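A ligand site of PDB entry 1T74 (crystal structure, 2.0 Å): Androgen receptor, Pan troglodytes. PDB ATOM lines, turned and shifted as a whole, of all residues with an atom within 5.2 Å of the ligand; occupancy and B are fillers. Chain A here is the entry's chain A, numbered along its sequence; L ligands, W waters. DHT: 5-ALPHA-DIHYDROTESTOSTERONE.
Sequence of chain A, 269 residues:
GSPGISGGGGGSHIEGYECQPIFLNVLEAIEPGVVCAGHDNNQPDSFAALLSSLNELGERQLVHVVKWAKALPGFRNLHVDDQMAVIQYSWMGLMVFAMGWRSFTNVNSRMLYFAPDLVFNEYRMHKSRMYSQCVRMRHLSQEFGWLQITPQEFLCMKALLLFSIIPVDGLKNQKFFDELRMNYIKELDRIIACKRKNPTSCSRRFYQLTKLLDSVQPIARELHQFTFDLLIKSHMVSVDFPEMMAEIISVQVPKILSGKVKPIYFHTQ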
ATOM      1  N   LEU A  51      13.814  -0.003  21.233  1.00  0.00           N
ATOM      2  CA  LEU A  51      12.556  -0.521  20.703  1.00  0.00           C
ATOM      3  C   LEU A  51      11.516  -0.823  21.781  1.00  0.00           C
ATOM      4  O   LEU A  51      10.319  -0.632  21.563  1.00  0.00           O
ATOM      5  CB  LEU A  51      12.830  -1.755  19.830  1.00  0.00           C
ATOM      6  CG  LEU A  51      13.105  -1.417  18.353  1.00  0.00           C
ATOM      7  CD1 LEU A  51      11.810  -0.947  17.724  1.00  0.00           C
ATOM      8  CD2 LEU A  51      14.193  -0.347  18.223  1.00  0.00           C
ATOM      9  N   LEU A  54      10.027   2.445  22.525  1.00  0.00           N
ATOM     10  CA  LEU A  54       9.196   2.918  21.415  1.00  0.00           C
ATOM     11  C   LEU A  54       7.852   2.186  21.464  1.00  0.00           C
ATOM     12  O   LEU A  54       6.800   2.751  21.152  1.00  0.00           O
ATOM     13  CB  LEU A  54       9.884   2.677  20.055  1.00  0.00           C
ATOM     14  CG  LEU A  54      10.962   3.677  19.614  1.00  0.00           C
ATOM     15  CD1 LEU A  54      11.547   3.210  18.287  1.00  0.00           C
ATOM     16  CD2 LEU A  54      10.355   5.079  19.459  1.00  0.00           C
ATOM     17  N   ASN A  55       7.884   0.921  21.873  1.00  0.00           N
ATOM     18  CA  ASN A  55       6.653   0.132  21.993  1.00  0.00           C
ATOM     19  C   ASN A  55       5.781   0.680  23.097  1.00  0.00           C
ATOM     20  O   ASN A  55       4.564   0.802  22.935  1.00  0.00           O
ATOM     21  CB  ASN A  55       6.962  -1.348  22.256  1.00  0.00           C
ATOM     22  CG  ASN A  55       7.489  -2.050  21.018  1.00  0.00           C
ATOM     23  OD1 ASN A  55       7.243  -1.614  19.896  1.00  0.00           O
ATOM     24  ND2 ASN A  55       8.203  -3.160  21.214  1.00  0.00           N
ATOM     25  N   LEU A  57       5.806   3.725  24.237  1.00  0.00           N
ATOM     26  CA  LEU A  57       5.301   5.031  23.800  1.00  0.00           C
ATOM     27  C   LEU A  57       4.065   4.803  22.936  1.00  0.00           C
ATOM     28  O   LEU A  57       3.057   5.495  23.076  1.00  0.00           O
ATOM     29  CB  LEU A  57       6.353   5.764  22.976  1.00  0.00           C
ATOM     30  CG  LEU A  57       5.900   7.124  22.436  1.00  0.00           C
ATOM     31  CD1 LEU A  57       5.496   8.041  23.595  1.00  0.00           C
ATOM     32  CD2 LEU A  57       7.024   7.751  21.615  1.00  0.00           C
ATOM     33  N   GLY A  58       4.154   3.835  22.030  1.00  0.00           N
ATOM     34  CA  GLY A  58       3.022   3.536  21.180  1.00  0.00           C
ATOM     35  C   GLY A  58       1.802   3.168  21.994  1.00  0.00           C
ATOM     36  O   GLY A  58       0.707   3.648  21.747  1.00  0.00           O
ATOM     37  N   GLN A  61       0.477   6.327  23.468  1.00  0.00           N
ATOM     38  CA  GLN A  61      -0.140   7.203  22.496  1.00  0.00           C
ATOM     39  C   GLN A  61      -1.426   6.588  21.968  1.00  0.00           C
ATOM     40  O   GLN A  61      -2.341   7.309  21.595  1.00  0.00           O
ATOM     41  CB  GLN A  61       0.834   7.495  21.339  1.00  0.00           C
ATOM     42  CG  GLN A  61       2.025   8.332  21.786  1.00  0.00           C
ATOM     43  CD  GLN A  61       2.736   8.999  20.636  1.00  0.00           C
ATOM     44  OE1 GLN A  61       3.770   9.660  20.835  1.00  0.00           O
ATOM     45  NE2 GLN A  61       2.198   8.850  19.439  1.00  0.00           N
ATOM     46  N   TRP A  91      -3.495   4.081  13.066  1.00  0.00           N
ATOM     47  CA  TRP A  91      -2.665   4.629  14.141  1.00  0.00           C
ATOM     48  C   TRP A  91      -1.208   4.885  13.782  1.00  0.00           C
ATOM     49  O   TRP A  91      -0.651   5.900  14.193  1.00  0.00           O
ATOM     50  CB  TRP A  91      -2.705   3.754  15.389  1.00  0.00           C
ATOM     51  CG  TRP A  91      -2.190   2.375  15.203  1.00  0.00           C
ATOM     52  CD1 TRP A  91      -2.895   1.279  14.822  1.00  0.00           C
ATOM     53  CD2 TRP A  91      -0.847   1.926  15.440  1.00  0.00           C
ATOM     54  NE1 TRP A  91      -2.084   0.167  14.820  1.00  0.00           N
ATOM     55  CE2 TRP A  91      -0.818   0.534  15.201  1.00  0.00           C
ATOM     56  CE3 TRP A  91       0.339   2.558  15.851  1.00  0.00           C
ATOM     57  CZ2 TRP A  91       0.334  -0.230  15.343  1.00  0.00           C
ATOM     58  CZ3 TRP A  91       1.491   1.794  15.993  1.00  0.00           C
ATOM     59  CH2 TRP A  91       1.478   0.417  15.745  1.00  0.00           C
ATOM     60  N   MET A  92      -0.593   3.989  13.030  1.00  0.00           N
ATOM     61  CA  MET A  92       0.811   4.160  12.678  1.00  0.00           C
ATOM     62  C   MET A  92       1.032   5.488  11.946  1.00  0.00           C
ATOM     63  O   MET A  92       1.889   6.283  12.350  1.00  0.00           O
ATOM     64  CB  MET A  92       1.304   3.018  11.787  1.00  0.00           C
ATOM     65  CG  MET A  92       2.791   3.101  11.457  1.00  0.00           C
ATOM     66  SD  MET A  92       3.863   2.736  12.882  1.00  0.00           S
ATOM     67  CE  MET A  92       3.856   0.944  12.835  1.00  0.00           C
ATOM     68  N   MET A  95       0.355   8.590  14.223  1.00  0.00           N
ATOM     69  CA  MET A  95       1.441   8.842  15.156  1.00  0.00           C
ATOM     70  C   MET A  95       2.730   9.342  14.475  1.00  0.00           C
ATOM     71  O   MET A  95       3.417  10.194  15.014  1.00  0.00           O
ATOM     72  CB  MET A  95       1.756   7.572  15.964  1.00  0.00           C
ATOM     73  CG  MET A  95       0.619   7.118  16.884  1.00  0.00           C
ATOM     74  SD  MET A  95       1.073   5.669  17.863  1.00  0.00           S
ATOM     75  CE  MET A  95      -0.546   5.290  18.675  1.00  0.00           C
ATOM     76  N   VAL A  96       3.050   8.800  13.308  1.00  0.00           N
ATOM     77  CA  VAL A  96       4.250   9.235  12.603  1.00  0.00           C
ATOM     78  C   VAL A  96       4.102  10.695  12.153  1.00  0.00           C
ATOM     79  O   VAL A  96       5.027  11.486  12.295  1.00  0.00           O
ATOM     80  CB  VAL A  96       4.533   8.329  11.358  1.00  0.00           C
ATOM     81  CG1 VAL A  96       5.580   8.979  10.445  1.00  0.00           C
ATOM     82  CG2 VAL A  96       5.031   6.966  11.810  1.00  0.00           C
ATOM     83  N   MET A  99       4.410  12.952  15.020  1.00  0.00           N
ATOM     84  CA  MET A  99       5.787  12.940  15.480  1.00  0.00           C
ATOM     85  C   MET A  99       6.602  13.862  14.569  1.00  0.00           C
ATOM     86  O   MET A  99       7.497  14.582  15.022  1.00  0.00           O
ATOM     87  CB  MET A  99       6.345  11.520  15.458  1.00  0.00           C
ATOM     88  CG  MET A  99       7.738  11.367  16.054  1.00  0.00           C
ATOM     89  SD  MET A  99       9.092  11.738  14.889  1.00  0.00           S
ATOM     90  CE  MET A  99       8.919  10.352  13.751  1.00  0.00           C
ATOM     91  N   ARG A 102       6.058  17.316  15.677  1.00  0.00           N
ATOM     92  CA  ARG A 102       6.784  17.603  16.916  1.00  0.00           C
ATOM     93  C   ARG A 102       8.252  17.868  16.638  1.00  0.00           C
ATOM     94  O   ARG A 102       8.844  18.796  17.196  1.00  0.00           O
ATOM     95  CB  ARG A 102       6.705  16.430  17.916  1.00  0.00           C
ATOM     96  CG  ARG A 102       5.366  16.259  18.582  1.00  0.00           C
ATOM     97  CD  ARG A 102       5.500  15.394  19.852  1.00  0.00           C
ATOM     98  NE  ARG A 102       5.850  14.004  19.564  1.00  0.00           N
ATOM     99  CZ  ARG A 102       5.013  13.112  19.037  1.00  0.00           C
ATOM    100  NH1 ARG A 102       3.774  13.458  18.718  1.00  0.00           N
ATOM    101  NH2 ARG A 102       5.405  11.854  18.865  1.00  0.00           N
ATOM    102  N   PHE A 114      10.346  11.774  19.159  1.00  0.00           N
ATOM    103  CA  PHE A 114       9.306  10.817  19.484  1.00  0.00           C
ATOM    104  C   PHE A 114       8.559  11.227  20.750  1.00  0.00           C
ATOM    105  O   PHE A 114       7.336  11.225  20.776  1.00  0.00           O
ATOM    106  CB  PHE A 114       9.909   9.423  19.644  1.00  0.00           C
ATOM    107  CG  PHE A 114      10.384   8.817  18.358  1.00  0.00           C
ATOM    108  CD1 PHE A 114       9.478   8.338  17.424  1.00  0.00           C
ATOM    109  CD2 PHE A 114      11.740   8.730  18.078  1.00  0.00           C
ATOM    110  CE1 PHE A 114       9.911   7.779  16.226  1.00  0.00           C
ATOM    111  CE2 PHE A 114      12.197   8.174  16.874  1.00  0.00           C
ATOM    112  CZ  PHE A 114      11.267   7.693  15.946  1.00  0.00           C
ATOM    113  N   MET A 130      16.555   0.822  12.353  1.00  0.00           N
ATOM    114  CA  MET A 130      15.564   1.343  11.414  1.00  0.00           C
ATOM    115  C   MET A 130      15.972   2.726  10.964  1.00  0.00           C
ATOM    116  O   MET A 130      15.192   3.672  10.988  1.00  0.00           O
ATOM    117  CB  MET A 130      14.158   1.337  12.037  1.00  0.00           C
ATOM    118  CG  MET A 130      14.066   1.788  13.473  1.00  0.00           C
ATOM    119  SD  MET A 130      12.339   1.714  14.059  1.00  0.00           S
ATOM    120  CE  MET A 130      11.875   3.438  13.980  1.00  0.00           C
ATOM    121  N   MET A 137      11.218   9.457   7.850  1.00  0.00           N
ATOM    122  CA  MET A 137      10.394  10.216   8.787  1.00  0.00           C
ATOM    123  C   MET A 137      10.972  11.628   8.933  1.00  0.00           C
ATOM    124  O   MET A 137      10.226  12.600   9.082  1.00  0.00           O
ATOM    125  CB  MET A 137      10.315   9.505  10.148  1.00  0.00           C
ATOM    126  CG  MET A 137       9.472   8.232  10.095  1.00  0.00           C
ATOM    127  SD  MET A 137       9.099   7.481  11.709  1.00  0.00           S
ATOM    128  CE  MET A 137      10.560   6.534  11.974  1.00  0.00           C
ATOM    129  N   LEU A 223       7.056   0.750   8.408  1.00  0.00           N
ATOM    130  CA  LEU A 223       7.028   0.578   9.843  1.00  0.00           C
ATOM    131  C   LEU A 223       6.138  -0.605  10.215  1.00  0.00           C
ATOM    132  O   LEU A 223       6.433  -1.341  11.146  1.00  0.00           O
ATOM    133  CB  LEU A 223       6.558   1.879  10.514  1.00  0.00           C
ATOM    134  CG  LEU A 223       7.580   3.023  10.355  1.00  0.00           C
ATOM    135  CD1 LEU A 223       6.989   4.330  10.827  1.00  0.00           C
ATOM    136  CD2 LEU A 223       8.846   2.688  11.140  1.00  0.00           C
ATOM    137  N   PHE A 226       8.162  -3.661   9.509  1.00  0.00           N
ATOM    138  CA  PHE A 226       9.226  -3.729  10.505  1.00  0.00           C
ATOM    139  C   PHE A 226       8.738  -4.184  11.883  1.00  0.00           C
ATOM    140  O   PHE A 226       9.345  -5.071  12.487  1.00  0.00           O
ATOM    141  CB  PHE A 226       9.906  -2.356  10.625  1.00  0.00           C
ATOM    142  CG  PHE A 226      11.114  -2.343  11.520  1.00  0.00           C
ATOM    143  CD1 PHE A 226      10.983  -2.142  12.886  1.00  0.00           C
ATOM    144  CD2 PHE A 226      12.387  -2.512  10.984  1.00  0.00           C
ATOM    145  CE1 PHE A 226      12.105  -2.099  13.708  1.00  0.00           C
ATOM    146  CE2 PHE A 226      13.521  -2.474  11.804  1.00  0.00           C
ATOM    147  CZ  PHE A 226      13.378  -2.267  13.172  1.00  0.00           C
ATOM    148  N   THR A 227       7.651  -3.602  12.369  1.00  0.00           N
ATOM    149  CA  THR A 227       7.138  -3.966  13.686  1.00  0.00           C
ATOM    150  C   THR A 227       6.547  -5.376  13.717  1.00  0.00           C
ATOM    151  O   THR A 227       6.623  -6.059  14.742  1.00  0.00           O
ATOM    152  CB  THR A 227       6.078  -2.942  14.182  1.00  0.00           C
ATOM    153  OG1 THR A 227       5.794  -3.191  15.559  1.00  0.00           O
ATOM    154  CG2 THR A 227       4.798  -3.027  13.369  1.00  0.00           C
ATOM    155  N   LEU A 230       9.440  -7.708  13.871  1.00  0.00           N
ATOM    156  CA  LEU A 230      10.020  -7.589  15.200  1.00  0.00           C
ATOM    157  C   LEU A 230       9.178  -8.327  16.243  1.00  0.00           C
ATOM    158  O   LEU A 230       9.716  -8.909  17.176  1.00  0.00           O
ATOM    159  CB  LEU A 230      10.157  -6.122  15.597  1.00  0.00           C
ATOM    160  CG  LEU A 230      10.778  -5.842  16.971  1.00  0.00           C
ATOM    161  CD1 LEU A 230      12.143  -6.503  17.076  1.00  0.00           C
ATOM    162  CD2 LEU A 230      10.890  -4.340  17.189  1.00  0.00           C
ATOM    163  N   PHE A 241       6.762  -6.042  23.959  1.00  0.00           N
ATOM    164  CA  PHE A 241       5.623  -5.433  23.284  1.00  0.00           C
ATOM    165  C   PHE A 241       4.457  -5.367  24.270  1.00  0.00           C
ATOM    166  O   PHE A 241       4.052  -6.387  24.830  1.00  0.00           O
ATOM    167  CB  PHE A 241       5.189  -6.267  22.067  1.00  0.00           C
ATOM    168  CG  PHE A 241       5.961  -5.962  20.808  1.00  0.00           C
ATOM    169  CD1 PHE A 241       7.196  -6.563  20.570  1.00  0.00           C
ATOM    170  CD2 PHE A 241       5.447  -5.093  19.853  1.00  0.00           C
ATOM    171  CE1 PHE A 241       7.912  -6.293  19.390  1.00  0.00           C
ATOM    172  CE2 PHE A 241       6.146  -4.810  18.681  1.00  0.00           C
ATOM    173  CZ  PHE A 241       7.381  -5.411  18.443  1.00  0.00           C
ATOM    174  N   ILE A 249      -0.862  -5.577  16.398  1.00  0.00           N
ATOM    175  CA  ILE A 249       0.158  -5.934  15.417  1.00  0.00           C
ATOM    176  C   ILE A 249       0.070  -7.371  14.907  1.00  0.00           C
ATOM    177  O   ILE A 249       0.529  -7.665  13.803  1.00  0.00           O
ATOM    178  CB  ILE A 249       1.567  -5.642  15.995  1.00  0.00           C
ATOM    179  CG1 ILE A 249       1.695  -4.141  16.257  1.00  0.00           C
ATOM    180  CG2 ILE A 249       2.644  -6.085  15.018  1.00  0.00           C
ATOM    181  CD1 ILE A 249       2.989  -3.713  16.905  1.00  0.00           C
HETATM  182  C1  DHT L   1       5.473   5.649  18.583  1.00  0.00           C
HETATM  183  C2  DHT L   1       4.737   6.994  18.594  1.00  0.00           C
HETATM  184  C3  DHT L   1       5.563   7.945  17.669  1.00  0.00           C
HETATM  185  O3  DHT L   1       5.908   9.015  18.124  1.00  0.00           O
HETATM  186  C4  DHT L   1       5.896   7.462  16.299  1.00  0.00           C
HETATM  187  C5  DHT L   1       6.654   6.104  16.350  1.00  0.00           C
HETATM  188  C6  DHT L   1       7.022   5.548  14.921  1.00  0.00           C
HETATM  189  C7  DHT L   1       7.801   4.233  15.069  1.00  0.00           C
HETATM  190  C8  DHT L   1       6.988   3.140  15.855  1.00  0.00           C
HETATM  191  C9  DHT L   1       6.594   3.698  17.266  1.00  0.00           C
HETATM  192  C10 DHT L   1       5.776   5.044  17.177  1.00  0.00           C
HETATM  193  C11 DHT L   1       5.808   2.580  18.048  1.00  0.00           C
HETATM  194  C12 DHT L   1       6.499   1.231  18.187  1.00  0.00           C
HETATM  195  C13 DHT L   1       7.021   0.689  16.832  1.00  0.00           C
HETATM  196  C14 DHT L   1       7.798   1.835  16.060  1.00  0.00           C
HETATM  197  C15 DHT L   1       8.282   1.098  14.808  1.00  0.00           C
HETATM  198  C16 DHT L   1       8.782  -0.244  15.389  1.00  0.00           C
HETATM  199  C17 DHT L   1       8.163  -0.316  16.823  1.00  0.00           C
HETATM  200  O17 DHT L   1       7.741  -1.656  17.091  1.00  0.00           O
HETATM  201  C18 DHT L   1       5.780   0.155  16.006  1.00  0.00           C
HETATM  202  C19 DHT L   1       4.397   4.766  16.427  1.00  0.00           C
HETATM  203  O   HOH W   1       2.952  10.683  17.671  1.00  0.00           O
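The side-chain amide nitrogen (NE2) of Gln 61 sits close to the side-chain sulfur (SD) of Met 95 (3.7 Å). The guanidinium group of Arg 102 is in hydrogen-bond range of the side-chain amide oxygen of Gln 61, at 3.4 Å. NH2 of Arg 102 lies within hydrogen-bond range of O of Phe 114. The side-chain amide nitrogen of Asn 55 sits close to the backbone carbonyl oxygen of Leu 51.
Leu 51 touches the ligand. O of Leu 54 touches C11 of the ligand (3.3 Å). CD2 of Leu 57 touches C2 of the ligand, 3.9 Å away. Gln 61 touches the ligand (NE2 to C2, 3.3 Å). Met 92 touches the ligand. SD of Met 95 touches C19 of the ligand, 3.7 Å away. CG2 of Val 96 touches C6 of the ligand, 3.96 Å away. Met 99 touches the ligand. Phe 114 touches the ligand. Phe 226 touches the ligand (CD1 to C16, 3.8 Å). Phe 241 touches the ligand. Hydrophobic or aromatic side chains within 4 Å of the ligand: Leu 51, Leu 57, Met 92, Met 95, Val 96, Met 99, Phe 114, Phe 226 and Phe 241. 14 residues have an atom within 4 Å of the ligand: Leu 51, Leu 54, Asn 55, Leu 57, Gln 61, Met 92, Met 95, Val 96, Met 99, Arg 102, Phe 114, Phe 226, Thr 227 and Phe 241.
OD1 of Asn 55 sits at hydrogen-bond distance from O17 of the ligand (2.8 Å). O3 of the ligand is in hydrogen-bond range of NH2 of Arg 102 (3.0 Å). OG1 of Thr 227 is in hydrogen-bond range of O17 of the ligand.
Water W1 lies within hydrogen-bond range of NE2 of Gln 61 (2.7 Å), O of Met 95 (2.7 Å), NH2 of Arg 102 (3.0 Å) and O3 of the ligand (3.4 Å).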
